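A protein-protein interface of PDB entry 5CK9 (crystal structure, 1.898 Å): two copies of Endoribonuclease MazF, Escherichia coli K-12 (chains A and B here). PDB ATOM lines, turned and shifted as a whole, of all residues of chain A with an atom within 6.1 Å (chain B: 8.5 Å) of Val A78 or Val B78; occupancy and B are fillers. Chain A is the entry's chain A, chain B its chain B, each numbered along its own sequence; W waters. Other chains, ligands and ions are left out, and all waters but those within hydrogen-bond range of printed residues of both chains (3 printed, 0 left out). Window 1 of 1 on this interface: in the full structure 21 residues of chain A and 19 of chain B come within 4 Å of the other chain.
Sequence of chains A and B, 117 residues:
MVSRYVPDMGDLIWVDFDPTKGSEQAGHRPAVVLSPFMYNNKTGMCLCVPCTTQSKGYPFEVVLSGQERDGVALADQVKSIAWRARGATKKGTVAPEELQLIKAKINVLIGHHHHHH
The side-chain carboxylate of Asp A76 is in hydrogen-bond range of the side-chain hydroxyl of Tyr B39 (2.5 Å).
The backbone carbonyl oxygen (O) of Val A78 lies within hydrogen-bond range of the backbone NH (N) of Ser B80 (3.0 Å).
The backbone NH (N) of Ser A80 sits at hydrogen-bond distance from the backbone carbonyl oxygen (O) of Val B78 (3.1 Å).
The backbone NH of Leu B47 lies within hydrogen-bond range of the side-chain hydroxyl of Ser B35, 3.0 Å away.
The backbone NH (N) of Leu A34 sits at hydrogen-bond distance from the backbone carbonyl oxygen (O) of Leu A47 (2.7 Å).
The backbone carbonyl oxygen (O) of Cys B48 is in hydrogen-bond range of the backbone NH (N) of Lys B79 (2.8 Å).
N of Leu B34 is in hydrogen-bond range of O of Leu B47, 2.8 Å away.
O of Cys A48 lies within hydrogen-bond range of N of Lys A79 (2.8 Å).
Among the printed residues, merely in contact across the chains: Leu A34 with Ile B110 (3.4 Å), Leu A47 with Asp B76 (3.3 Å), Leu A47 with Val B78 (3.9 Å), Leu A47 with Ile B110 (3.3 Å), Asp A76 with Leu B47 (3.3 Å), Asp A76 with Ser B80 (3.9 Å), Gln A77 with Ser B80 (3.8 Å), Val A78 with Val B78 (3.7 Å), Val A78 with Lys B79 (3.5 Å), Lys A79 with Val B78 (3.8 Å), Lys A79 with Ser B80 (3.5 Å), Ser A80 with Gln B77 (3.5 Å), Ile A110 with Leu B34 (3.7 Å), Ile A110 with Leu B47 (3.4 Å) and Ile A110 with Lys B103 (3.9 Å).
Val A78 touches just these residues of chain B: Val B78, Lys B79 and Ser B80.
Of chain A, only Leu A47, Val A78, Lys A79 and Ser A80 come within 4 Å of Val B78.
Printed residues of chain A within 4 Å of Leu B34: Ile A110 (3.7 Å).
Of the printed residues of chain A, Leu B47 touches Asp A76 and Ile A110.
Cys A48 touches none of the printed residues of chain B.
The nearest residue of chain B that does not touch Val A78 is Leu B47 (4.1 Å).
The nearest printed residue of chain B that does not touch Leu A47 is Leu B109 (4.2 Å).
Of the 14 printed residues of chain A, 8 touch a printed residue of chain B.
Printed residues of chain A that touch a printed residue of chain B: Leu A34, Leu A47, Asp A76, Gln A77, Val A78, Lys A79, Ser A80 and Ile A110.
Of the 25 printed residues of chain B, 10 touch a printed residue of chain A.
Among the printed residues, 18 pairs touch across the chains.
Among the printed residues, no Asp or Glu carboxylate lies within 4 Å of a Lys or Arg side-chain nitrogen of the other chain.
Leu A34 touches Ile B110, and with the chains exchanged Ile A110 touches Leu B34.
Leu A47 touches Asp B76, and with the chains exchanged Asp A76 touches Leu B47.
Leu A47 touches Ile B110, and with the chains exchanged Ile A110 touches Leu B47.
Asp A76 touches Ser B80, but with the chains exchanged Ser A80 does not touch Asp B76 (4.01 Å).
Of the 18 pairs that touch across the chains among the printed residues, 13 have their exchanged pair printed and touching as well.
Water W1 lies within hydrogen-bond range of OG of Ser B80, O of Asp A76 and OH of Tyr B39.
Water W3 bridges the side-chain hydroxyl of Ser A80 (2.7 Å) and the backbone carbonyl oxygen of Asp B76 (2.8 Å).
Water W2 lies within hydrogen-bond range of the backbone carbonyl oxygen of Ser A80 (3.2 Å) and the side-chain amide oxygen of Gln B77 (3.5 Å).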
ATOM      1  N   LEU A  34      16.592 -17.022 -16.876  1.00  0.00           N
ATOM      2  CA  LEU A  34      16.676 -17.614 -18.218  1.00  0.00           C
ATOM      3  C   LEU A  34      15.366 -17.546 -19.004  1.00  0.00           C
ATOM      4  O   LEU A  34      15.374 -17.493 -20.231  1.00  0.00           O
ATOM      5  CB  LEU A  34      17.140 -19.075 -18.131  1.00  0.00           C
ATOM      6  CG  LEU A  34      18.436 -19.351 -17.363  1.00  0.00           C
ATOM      7  CD1 LEU A  34      18.661 -20.865 -17.212  1.00  0.00           C
ATOM      8  CD2 LEU A  34      19.632 -18.664 -18.031  1.00  0.00           C
ATOM      9  N   LEU A  47      12.808 -19.669 -14.561  1.00  0.00           N
ATOM     10  CA  LEU A  47      13.971 -20.531 -14.566  1.00  0.00           C
ATOM     11  C   LEU A  47      15.181 -19.617 -14.407  1.00  0.00           C
ATOM     12  O   LEU A  47      15.260 -18.574 -15.050  1.00  0.00           O
ATOM     13  CB  LEU A  47      14.078 -21.299 -15.888  1.00  0.00           C
ATOM     14  CG  LEU A  47      13.035 -22.422 -16.054  1.00  0.00           C
ATOM     15  CD1 LEU A  47      13.174 -23.102 -17.410  1.00  0.00           C
ATOM     16  CD2 LEU A  47      13.201 -23.439 -14.933  1.00  0.00           C
ATOM     17  N   CYS A  48      16.113 -20.001 -13.544  1.00  0.00           N
ATOM     18  CA  CYS A  48      17.280 -19.165 -13.298  1.00  0.00           C
ATOM     19  C   CYS A  48      18.445 -20.050 -12.885  1.00  0.00           C
ATOM     20  O   CYS A  48      18.263 -21.251 -12.625  1.00  0.00           O
ATOM     21  CB  CYS A  48      16.971 -18.122 -12.213  1.00  0.00           C
ATOM     22  SG  CYS A  48      16.772 -18.787 -10.533  1.00  0.00           S
ATOM     23  N   VAL A  49      19.645 -19.476 -12.863  1.00  0.00           N
ATOM     24  CA  VAL A  49      20.803 -20.180 -12.325  1.00  0.00           C
ATOM     25  C   VAL A  49      21.453 -19.296 -11.276  1.00  0.00           C
ATOM     26  O   VAL A  49      21.490 -18.074 -11.435  1.00  0.00           O
ATOM     27  CB  VAL A  49      21.834 -20.577 -13.419  1.00  0.00           C
ATOM     28  CG1 VAL A  49      21.217 -21.590 -14.396  1.00  0.00           C
ATOM     29  CG2 VAL A  49      22.368 -19.346 -14.149  1.00  0.00           C
ATOM     30  N   PRO A  50      21.941 -19.912 -10.193  1.00  0.00           N
ATOM     31  CA  PRO A  50      22.516 -19.158  -9.077  1.00  0.00           C
ATOM     32  C   PRO A  50      23.914 -18.674  -9.414  1.00  0.00           C
ATOM     33  O   PRO A  50      24.564 -19.248 -10.294  1.00  0.00           O
ATOM     34  CB  PRO A  50      22.567 -20.187  -7.942  1.00  0.00           C
ATOM     35  CG  PRO A  50      22.698 -21.524  -8.658  1.00  0.00           C
ATOM     36  CD  PRO A  50      21.967 -21.372  -9.965  1.00  0.00           C
ATOM     37  N   LEU A  74      26.386 -20.475 -12.194  1.00  0.00           N
ATOM     38  CA  LEU A  74      26.587 -21.918 -12.219  1.00  0.00           C
ATOM     39  C   LEU A  74      25.531 -22.517 -13.134  1.00  0.00           C
ATOM     40  O   LEU A  74      24.417 -22.781 -12.705  1.00  0.00           O
ATOM     41  CB  LEU A  74      26.483 -22.495 -10.808  1.00  0.00           C
ATOM     42  CG  LEU A  74      27.544 -21.976  -9.825  1.00  0.00           C
ATOM     43  CD1 LEU A  74      27.287 -22.509  -8.422  1.00  0.00           C
ATOM     44  CD2 LEU A  74      28.938 -22.366 -10.296  1.00  0.00           C
ATOM     45  N   ALA A  75      25.897 -22.719 -14.395  1.00  0.00           N
ATOM     46  CA  ALA A  75      24.927 -22.986 -15.445  1.00  0.00           C
ATOM     47  C   ALA A  75      24.216 -24.326 -15.276  1.00  0.00           C
ATOM     48  O   ALA A  75      23.080 -24.469 -15.710  1.00  0.00           O
ATOM     49  CB  ALA A  75      25.577 -22.909 -16.806  1.00  0.00           C
ATOM     50  N   ASP A  76      24.882 -25.299 -14.656  1.00  0.00           N
ATOM     51  CA  ASP A  76      24.254 -26.613 -14.447  1.00  0.00           C
ATOM     52  C   ASP A  76      23.196 -26.590 -13.341  1.00  0.00           C
ATOM     53  O   ASP A  76      22.362 -27.495 -13.249  1.00  0.00           O
ATOM     54  CB  ASP A  76      25.306 -27.707 -14.183  1.00  0.00           C
ATOM     55  CG  ASP A  76      26.144 -27.446 -12.927  1.00  0.00           C
ATOM     56  OD1 ASP A  76      26.447 -26.264 -12.648  1.00  0.00           O
ATOM     57  OD2 ASP A  76      26.511 -28.424 -12.226  1.00  0.00           O
ATOM     58  N   GLN A  77      23.202 -25.549 -12.515  1.00  0.00           N
ATOM     59  CA  GLN A  77      22.301 -25.528 -11.362  1.00  0.00           C
ATOM     60  C   GLN A  77      20.990 -24.794 -11.635  1.00  0.00           C
ATOM     61  O   GLN A  77      20.555 -23.967 -10.834  1.00  0.00           O
ATOM     62  CB  GLN A  77      22.999 -24.952 -10.126  1.00  0.00           C
ATOM     63  CG  GLN A  77      24.210 -25.756  -9.678  1.00  0.00           C
ATOM     64  CD  GLN A  77      24.592 -25.473  -8.238  1.00  0.00           C
ATOM     65  OE1 GLN A  77      23.748 -25.115  -7.415  1.00  0.00           O
ATOM     66  NE2 GLN A  77      25.871 -25.633  -7.926  1.00  0.00           N
ATOM     67  N   VAL A  78      20.364 -25.105 -12.764  1.00  0.00           N
ATOM     68  CA  VAL A  78      19.067 -24.529 -13.106  1.00  0.00           C
ATOM     69  C   VAL A  78      18.055 -24.735 -11.987  1.00  0.00           C
ATOM     70  O   VAL A  78      17.950 -25.821 -11.429  1.00  0.00           O
ATOM     71  CB  VAL A  78      18.472 -25.177 -14.369  1.00  0.00           C
ATOM     72  CG1 VAL A  78      17.102 -24.574 -14.665  1.00  0.00           C
ATOM     73  CG2 VAL A  78      19.411 -25.009 -15.552  1.00  0.00           C
ATOM     74  N   LYS A  79      17.306 -23.685 -11.670  1.00  0.00           N
ATOM     75  CA  LYS A  79      16.290 -23.749 -10.631  1.00  0.00           C
ATOM     76  C   LYS A  79      15.009 -23.108 -11.155  1.00  0.00           C
ATOM     77  O   LYS A  79      15.056 -22.042 -11.751  1.00  0.00           O
ATOM     78  CB  LYS A  79      16.739 -22.978  -9.386  1.00  0.00           C
ATOM     79  CG  LYS A  79      18.188 -23.193  -8.957  1.00  0.00           C
ATOM     80  CD  LYS A  79      18.365 -24.426  -8.085  1.00  0.00           C
ATOM     81  CE  LYS A  79      19.838 -24.638  -7.723  1.00  0.00           C
ATOM     82  NZ  LYS A  79      20.075 -25.908  -6.966  1.00  0.00           N
ATOM     83  N   SER A  80      13.870 -23.756 -10.920  1.00  0.00           N
ATOM     84  CA  SER A  80      12.567 -23.154 -11.170  1.00  0.00           C
ATOM     85  C   SER A  80      12.136 -22.558  -9.838  1.00  0.00           C
ATOM     86  O   SER A  80      11.969 -23.285  -8.874  1.00  0.00           O
ATOM     87  CB  SER A  80      11.551 -24.250 -11.588  1.00  0.00           C
ATOM     88  OG  SER A  80      10.251 -23.701 -11.752  1.00  0.00           O
ATOM     89  N   ILE A 106      23.880 -25.402 -20.580  1.00  0.00           N
ATOM     90  CA  ILE A 106      22.700 -26.198 -20.223  1.00  0.00           C
ATOM     91  C   ILE A 106      22.372 -27.194 -21.330  1.00  0.00           C
ATOM     92  O   ILE A 106      22.033 -28.355 -21.065  1.00  0.00           O
ATOM     93  CB  ILE A 106      21.481 -25.298 -19.903  1.00  0.00           C
ATOM     94  CG1 ILE A 106      21.744 -24.498 -18.618  1.00  0.00           C
ATOM     95  CG2 ILE A 106      20.202 -26.133 -19.750  1.00  0.00           C
ATOM     96  CD1 ILE A 106      20.804 -23.311 -18.421  1.00  0.00           C
ATOM     97  N   ILE A 110      21.741 -31.305 -20.966  1.00  0.00           N
ATOM     98  CA  ILE A 110      20.456 -31.965 -21.173  1.00  0.00           C
ATOM     99  C   ILE A 110      20.096 -32.148 -22.650  1.00  0.00           C
ATOM    100  O   ILE A 110      19.626 -31.222 -23.313  1.00  0.00           O
ATOM    101  CB  ILE A 110      19.328 -31.270 -20.386  1.00  0.00           C
ATOM    102  CG1 ILE A 110      19.182 -29.810 -20.799  1.00  0.00           C
ATOM    103  CG2 ILE A 110      19.618 -31.337 -18.900  1.00  0.00           C
ATOM    104  CD1 ILE A 110      18.223 -29.020 -19.919  1.00  0.00           C
ATOM    105  N   PHE B  17      11.157 -34.550  -2.018  1.00  0.00           N
ATOM    106  CA  PHE B  17      11.057 -33.154  -2.445  1.00  0.00           C
ATOM    107  C   PHE B  17      10.820 -32.179  -1.288  1.00  0.00           C
ATOM    108  O   PHE B  17      10.366 -31.058  -1.507  1.00  0.00           O
ATOM    109  CB  PHE B  17       9.946 -32.988  -3.487  1.00  0.00           C
ATOM    110  CG  PHE B  17      10.414 -33.135  -4.910  1.00  0.00           C
ATOM    111  CD1 PHE B  17      10.189 -34.306  -5.614  1.00  0.00           C
ATOM    112  CD2 PHE B  17      11.079 -32.098  -5.542  1.00  0.00           C
ATOM    113  CE1 PHE B  17      10.618 -34.437  -6.922  1.00  0.00           C
ATOM    114  CE2 PHE B  17      11.508 -32.226  -6.850  1.00  0.00           C
ATOM    115  CZ  PHE B  17      11.279 -33.395  -7.540  1.00  0.00           C
ATOM    116  N   VAL B  32      11.404 -36.794 -13.725  1.00  0.00           N
ATOM    117  CA  VAL B  32      12.080 -37.338 -14.898  1.00  0.00           C
ATOM    118  C   VAL B  32      13.497 -36.785 -14.980  1.00  0.00           C
ATOM    119  O   VAL B  32      13.682 -35.572 -14.984  1.00  0.00           O
ATOM    120  CB  VAL B  32      11.321 -37.004 -16.211  1.00  0.00           C
ATOM    121  CG1 VAL B  32      12.092 -37.542 -17.418  1.00  0.00           C
ATOM    122  CG2 VAL B  32       9.903 -37.610 -16.189  1.00  0.00           C
ATOM    123  N   LEU B  34      16.926 -35.605 -16.584  1.00  0.00           N
ATOM    124  CA  LEU B  34      17.275 -35.033 -17.885  1.00  0.00           C
ATOM    125  C   LEU B  34      18.774 -35.096 -18.177  1.00  0.00           C
ATOM    126  O   LEU B  34      19.186 -35.124 -19.332  1.00  0.00           O
ATOM    127  CB  LEU B  34      16.793 -33.575 -17.977  1.00  0.00           C
ATOM    128  CG  LEU B  34      15.294 -33.323 -17.776  1.00  0.00           C
ATOM    129  CD1 LEU B  34      14.993 -31.833 -17.761  1.00  0.00           C
ATOM    130  CD2 LEU B  34      14.479 -34.030 -18.839  1.00  0.00           C
ATOM    131  N   SER B  35      19.585 -35.112 -17.130  1.00  0.00           N
ATOM    132  CA  SER B  35      21.040 -35.086 -17.287  1.00  0.00           C
ATOM    133  C   SER B  35      21.610 -36.506 -17.357  1.00  0.00           C
ATOM    134  O   SER B  35      20.992 -37.440 -16.855  1.00  0.00           O
ATOM    135  CB  SER B  35      21.665 -34.320 -16.126  1.00  0.00           C
ATOM    136  OG  SER B  35      21.193 -34.847 -14.896  1.00  0.00           O
ATOM    137  N   TYR B  39      27.387 -37.155 -15.518  1.00  0.00           N
ATOM    138  CA  TYR B  39      27.176 -35.973 -14.700  1.00  0.00           C
ATOM    139  C   TYR B  39      26.561 -36.333 -13.355  1.00  0.00           C
ATOM    140  O   TYR B  39      27.056 -35.930 -12.304  1.00  0.00           O
ATOM    141  CB  TYR B  39      26.266 -34.967 -15.409  1.00  0.00           C
ATOM    142  CG  TYR B  39      25.932 -33.778 -14.530  1.00  0.00           C
ATOM    143  CD1 TYR B  39      26.780 -32.683 -14.476  1.00  0.00           C
ATOM    144  CD2 TYR B  39      24.778 -33.757 -13.746  1.00  0.00           C
ATOM    145  CE1 TYR B  39      26.496 -31.593 -13.672  1.00  0.00           C
ATOM    146  CE2 TYR B  39      24.485 -32.669 -12.931  1.00  0.00           C
ATOM    147  CZ  TYR B  39      25.358 -31.588 -12.905  1.00  0.00           C
ATOM    148  OH  TYR B  39      25.090 -30.500 -12.105  1.00  0.00           O
ATOM    149  N   CYS B  46      21.404 -33.968 -10.261  1.00  0.00           N
ATOM    150  CA  CYS B  46      20.864 -34.189 -11.591  1.00  0.00           C
ATOM    151  C   CYS B  46      19.868 -33.094 -11.920  1.00  0.00           C
ATOM    152  O   CYS B  46      19.326 -32.446 -11.023  1.00  0.00           O
ATOM    153  CB  CYS B  46      20.195 -35.579 -11.701  1.00  0.00           C
ATOM    154  SG  CYS B  46      18.739 -35.776 -10.635  1.00  0.00           S
ATOM    155  N   LEU B  47      19.650 -32.862 -13.207  1.00  0.00           N
ATOM    156  CA  LEU B  47      18.584 -31.964 -13.624  1.00  0.00           C
ATOM    157  C   LEU B  47      17.376 -32.858 -13.852  1.00  0.00           C
ATOM    158  O   LEU B  47      17.506 -33.916 -14.442  1.00  0.00           O
ATOM    159  CB  LEU B  47      18.953 -31.227 -14.912  1.00  0.00           C
ATOM    160  CG  LEU B  47      19.990 -30.110 -14.760  1.00  0.00           C
ATOM    161  CD1 LEU B  47      20.291 -29.476 -16.116  1.00  0.00           C
ATOM    162  CD2 LEU B  47      19.471 -29.070 -13.796  1.00  0.00           C
ATOM    163  N   CYS B  48      16.217 -32.444 -13.356  1.00  0.00           N
ATOM    164  CA  CYS B  48      15.005 -33.252 -13.502  1.00  0.00           C
ATOM    165  C   CYS B  48      13.796 -32.328 -13.621  1.00  0.00           C
ATOM    166  O   CYS B  48      13.925 -31.106 -13.430  1.00  0.00           O
ATOM    167  CB  CYS B  48      14.873 -34.212 -12.317  1.00  0.00           C
ATOM    168  SG  CYS B  48      14.529 -33.442 -10.729  1.00  0.00           S
ATOM    169  N   VAL B  49      12.647 -32.892 -13.996  1.00  0.00           N
ATOM    170  CA  VAL B  49      11.384 -32.174 -13.934  1.00  0.00           C
ATOM    171  C   VAL B  49      10.403 -33.017 -13.125  1.00  0.00           C
ATOM    172  O   VAL B  49      10.370 -34.241 -13.276  1.00  0.00           O
ATOM    173  CB  VAL B  49      10.807 -31.866 -15.336  1.00  0.00           C
ATOM    174  CG1 VAL B  49      11.726 -30.865 -16.092  1.00  0.00           C
ATOM    175  CG2 VAL B  49      10.624 -33.145 -16.125  1.00  0.00           C
ATOM    176  N   PRO B  50       9.631 -32.365 -12.241  1.00  0.00           N
ATOM    177  CA  PRO B  50       8.693 -33.076 -11.368  1.00  0.00           C
ATOM    178  C   PRO B  50       7.520 -33.623 -12.161  1.00  0.00           C
ATOM    179  O   PRO B  50       7.194 -33.100 -13.236  1.00  0.00           O
ATOM    180  CB  PRO B  50       8.208 -31.983 -10.408  1.00  0.00           C
ATOM    181  CG  PRO B  50       8.379 -30.705 -11.185  1.00  0.00           C
ATOM    182  CD  PRO B  50       9.620 -30.909 -11.994  1.00  0.00           C
ATOM    183  N   LEU B  74       6.085 -31.923 -15.668  1.00  0.00           N
ATOM    184  CA  LEU B  74       5.952 -30.471 -15.773  1.00  0.00           C
ATOM    185  C   LEU B  74       7.251 -29.927 -16.322  1.00  0.00           C
ATOM    186  O   LEU B  74       8.178 -29.649 -15.568  1.00  0.00           O
ATOM    187  CB  LEU B  74       5.651 -29.873 -14.399  1.00  0.00           C
ATOM    188  CG  LEU B  74       4.393 -30.472 -13.749  1.00  0.00           C
ATOM    189  CD1 LEU B  74       4.118 -29.868 -12.379  1.00  0.00           C
ATOM    190  CD2 LEU B  74       3.203 -30.288 -14.677  1.00  0.00           C
ATOM    191  N   ALA B  75       7.319 -29.805 -17.643  1.00  0.00           N
ATOM    192  CA  ALA B  75       8.580 -29.541 -18.331  1.00  0.00           C
ATOM    193  C   ALA B  75       9.212 -28.194 -17.983  1.00  0.00           C
ATOM    194  O   ALA B  75      10.426 -28.051 -18.071  1.00  0.00           O
ATOM    195  CB  ALA B  75       8.403 -29.676 -19.838  1.00  0.00           C
ATOM    196  N   ASP B  76       8.399 -27.215 -17.586  1.00  0.00           N
ATOM    197  CA  ASP B  76       8.925 -25.886 -17.259  1.00  0.00           C
ATOM    198  C   ASP B  76       9.579 -25.868 -15.881  1.00  0.00           C
ATOM    199  O   ASP B  76      10.345 -24.953 -15.560  1.00  0.00           O
ATOM    200  CB  ASP B  76       7.821 -24.814 -17.334  1.00  0.00           C
ATOM    201  CG  ASP B  76       6.648 -25.103 -16.391  1.00  0.00           C
ATOM    202  OD1 ASP B  76       6.307 -26.304 -16.213  1.00  0.00           O
ATOM    203  OD2 ASP B  76       6.073 -24.131 -15.832  1.00  0.00           O
ATOM    204  N   GLN B  77       9.282 -26.875 -15.066  1.00  0.00           N
ATOM    205  CA  GLN B  77       9.757 -26.864 -13.688  1.00  0.00           C
ATOM    206  C   GLN B  77      11.092 -27.577 -13.521  1.00  0.00           C
ATOM    207  O   GLN B  77      11.281 -28.367 -12.592  1.00  0.00           O
ATOM    208  CB  GLN B  77       8.706 -27.451 -12.748  1.00  0.00           C
ATOM    209  CG  GLN B  77       7.381 -26.725 -12.823  1.00  0.00           C
ATOM    210  CD  GLN B  77       6.882 -26.301 -11.465  1.00  0.00           C
ATOM    211  OE1 GLN B  77       7.124 -25.177 -11.026  1.00  0.00           O
ATOM    212  NE2 GLN B  77       6.190 -27.200 -10.784  1.00  0.00           N
ATOM    213  N   VAL B  78      12.025 -27.275 -14.418  1.00  0.00           N
ATOM    214  CA  VAL B  78      13.347 -27.874 -14.372  1.00  0.00           C
ATOM    215  C   VAL B  78      13.982 -27.555 -13.036  1.00  0.00           C
ATOM    216  O   VAL B  78      13.902 -26.423 -12.568  1.00  0.00           O
ATOM    217  CB  VAL B  78      14.260 -27.282 -15.444  1.00  0.00           C
ATOM    218  CG1 VAL B  78      15.628 -27.939 -15.381  1.00  0.00           C
ATOM    219  CG2 VAL B  78      13.639 -27.446 -16.809  1.00  0.00           C
ATOM    220  N   LYS B  79      14.619 -28.542 -12.415  1.00  0.00           N
ATOM    221  CA  LYS B  79      15.384 -28.243 -11.213  1.00  0.00           C
ATOM    222  C   LYS B  79      16.593 -29.145 -11.008  1.00  0.00           C
ATOM    223  O   LYS B  79      16.595 -30.308 -11.402  1.00  0.00           O
ATOM    224  CB  LYS B  79      14.488 -28.218  -9.973  1.00  0.00           C
ATOM    225  CG  LYS B  79      13.663 -29.446  -9.751  1.00  0.00           C
ATOM    226  CD  LYS B  79      12.488 -29.135  -8.833  1.00  0.00           C
ATOM    227  N   SER B  80      17.624 -28.570 -10.404  1.00  0.00           N
ATOM    228  CA  SER B  80      18.845 -29.270 -10.058  1.00  0.00           C
ATOM    229  C   SER B  80      18.677 -29.778  -8.636  1.00  0.00           C
ATOM    230  O   SER B  80      18.480 -28.990  -7.712  1.00  0.00           O
ATOM    231  CB  SER B  80      20.037 -28.281 -10.112  1.00  0.00           C
ATOM    232  OG  SER B  80      21.257 -28.944  -9.822  1.00  0.00           O
ATOM    233  N   ILE B  81      18.760 -31.089  -8.439  1.00  0.00           N
ATOM    234  CA  ILE B  81      18.625 -31.633  -7.089  1.00  0.00           C
ATOM    235  C   ILE B  81      19.750 -32.573  -6.728  1.00  0.00           C
ATOM    236  O   ILE B  81      20.381 -33.173  -7.596  1.00  0.00           O
ATOM    237  CB  ILE B  81      17.306 -32.405  -6.909  1.00  0.00           C
ATOM    238  CG1 ILE B  81      17.241 -33.575  -7.894  1.00  0.00           C
ATOM    239  CG2 ILE B  81      16.143 -31.467  -7.079  1.00  0.00           C
ATOM    240  CD1 ILE B  81      16.248 -34.668  -7.495  1.00  0.00           C
ATOM    241  N   ILE B 102       9.675 -33.389 -23.604  1.00  0.00           N
ATOM    242  CA  ILE B 102      10.012 -32.588 -22.435  1.00  0.00           C
ATOM    243  C   ILE B 102      11.119 -31.602 -22.790  1.00  0.00           C
ATOM    244  O   ILE B 102      11.075 -30.429 -22.407  1.00  0.00           O
ATOM    245  CB  ILE B 102      10.436 -33.462 -21.224  1.00  0.00           C
ATOM    246  CG1 ILE B 102       9.218 -34.205 -20.650  1.00  0.00           C
ATOM    247  CG2 ILE B 102      11.149 -32.582 -20.148  1.00  0.00           C
ATOM    248  CD1 ILE B 102       9.586 -35.339 -19.703  1.00  0.00           C
ATOM    249  N   LYS B 103      12.115 -32.071 -23.533  1.00  0.00           N
ATOM    250  CA  LYS B 103      13.257 -31.226 -23.870  1.00  0.00           C
ATOM    251  C   LYS B 103      12.833 -30.146 -24.849  1.00  0.00           C
ATOM    252  O   LYS B 103      13.294 -29.008 -24.776  1.00  0.00           O
ATOM    253  CB  LYS B 103      14.394 -32.061 -24.463  1.00  0.00           C
ATOM    254  CG  LYS B 103      15.091 -32.933 -23.433  1.00  0.00           C
ATOM    255  CD  LYS B 103      16.172 -33.783 -24.065  1.00  0.00           C
ATOM    256  CE  LYS B 103      17.004 -34.460 -22.987  1.00  0.00           C
ATOM    257  NZ  LYS B 103      18.073 -35.298 -23.594  1.00  0.00           N
ATOM    258  N   LYS B 105       9.923 -28.716 -25.048  1.00  0.00           N
ATOM    259  CA  LYS B 105       9.196 -27.671 -24.323  1.00  0.00           C
ATOM    260  C   LYS B 105      10.114 -26.802 -23.462  1.00  0.00           C
ATOM    261  O   LYS B 105       9.921 -25.584 -23.366  1.00  0.00           O
ATOM    262  CB  LYS B 105       8.052 -28.262 -23.489  1.00  0.00           C
ATOM    263  CG  LYS B 105       6.927 -28.837 -24.348  1.00  0.00           C
ATOM    264  CD  LYS B 105       5.651 -29.104 -23.550  1.00  0.00           C
ATOM    265  CE  LYS B 105       4.472 -29.351 -24.502  1.00  0.00           C
ATOM    266  NZ  LYS B 105       3.247 -29.814 -23.792  1.00  0.00           N
ATOM    267  N   ILE B 106      11.115 -27.412 -22.836  1.00  0.00           N
ATOM    268  CA  ILE B 106      12.133 -26.603 -22.144  1.00  0.00           C
ATOM    269  C   ILE B 106      12.806 -25.635 -23.112  1.00  0.00           C
ATOM    270  O   ILE B 106      13.013 -24.455 -22.804  1.00  0.00           O
ATOM    271  CB  ILE B 106      13.198 -27.483 -21.458  1.00  0.00           C
ATOM    272  CG1 ILE B 106      12.548 -28.311 -20.335  1.00  0.00           C
ATOM    273  CG2 ILE B 106      14.355 -26.609 -20.928  1.00  0.00           C
ATOM    274  CD1 ILE B 106      13.400 -29.476 -19.811  1.00  0.00           C
ATOM    275  N   ASN B 107      13.141 -26.132 -24.296  1.00  0.00           N
ATOM    276  CA  ASN B 107      13.841 -25.316 -25.279  1.00  0.00           C
ATOM    277  C   ASN B 107      12.995 -24.138 -25.763  1.00  0.00           C
ATOM    278  O   ASN B 107      13.519 -23.084 -26.152  1.00  0.00           O
ATOM    279  CB  ASN B 107      14.289 -26.182 -26.459  1.00  0.00           C
ATOM    280  CG  ASN B 107      15.517 -25.624 -27.152  1.00  0.00           C
ATOM    281  OD1 ASN B 107      15.421 -25.050 -28.235  1.00  0.00           O
ATOM    282  ND2 ASN B 107      16.683 -25.786 -26.524  1.00  0.00           N
ATOM    283  N   LEU B 109      11.102 -22.491 -23.851  1.00  0.00           N
ATOM    284  CA  LEU B 109      11.160 -21.532 -22.759  1.00  0.00           C
ATOM    285  C   LEU B 109      12.551 -20.907 -22.622  1.00  0.00           C
ATOM    286  O   LEU B 109      12.696 -19.701 -22.400  1.00  0.00           O
ATOM    287  CB  LEU B 109      10.771 -22.242 -21.456  1.00  0.00           C
ATOM    288  CG  LEU B 109      10.032 -21.439 -20.385  1.00  0.00           C
ATOM    289  CD1 LEU B 109       8.936 -20.558 -21.001  1.00  0.00           C
ATOM    290  CD2 LEU B 109       9.456 -22.387 -19.338  1.00  0.00           C
ATOM    291  N   ILE B 110      13.578 -21.729 -22.791  1.00  0.00           N
ATOM    292  CA  ILE B 110      14.936 -21.347 -22.417  1.00  0.00           C
ATOM    293  C   ILE B 110      15.936 -21.488 -23.567  1.00  0.00           C
ATOM    294  O   ILE B 110      17.140 -21.279 -23.385  1.00  0.00           O
ATOM    295  CB  ILE B 110      15.377 -22.175 -21.188  1.00  0.00           C
ATOM    296  CG1 ILE B 110      15.301 -21.312 -19.931  1.00  0.00           C
ATOM    297  CG2 ILE B 110      16.742 -22.818 -21.390  1.00  0.00           C
ATOM    298  CD1 ILE B 110      13.907 -20.788 -19.666  1.00  0.00           C
HETATM  299  O   HOH W   1      22.250 -29.918 -11.790  1.00  0.00           O
HETATM  300  O   HOH W   2       9.769 -25.601  -8.793  1.00  0.00           O
HETATM  301  O   HOH W   3       9.885 -22.539 -14.180  1.00  0.00           O
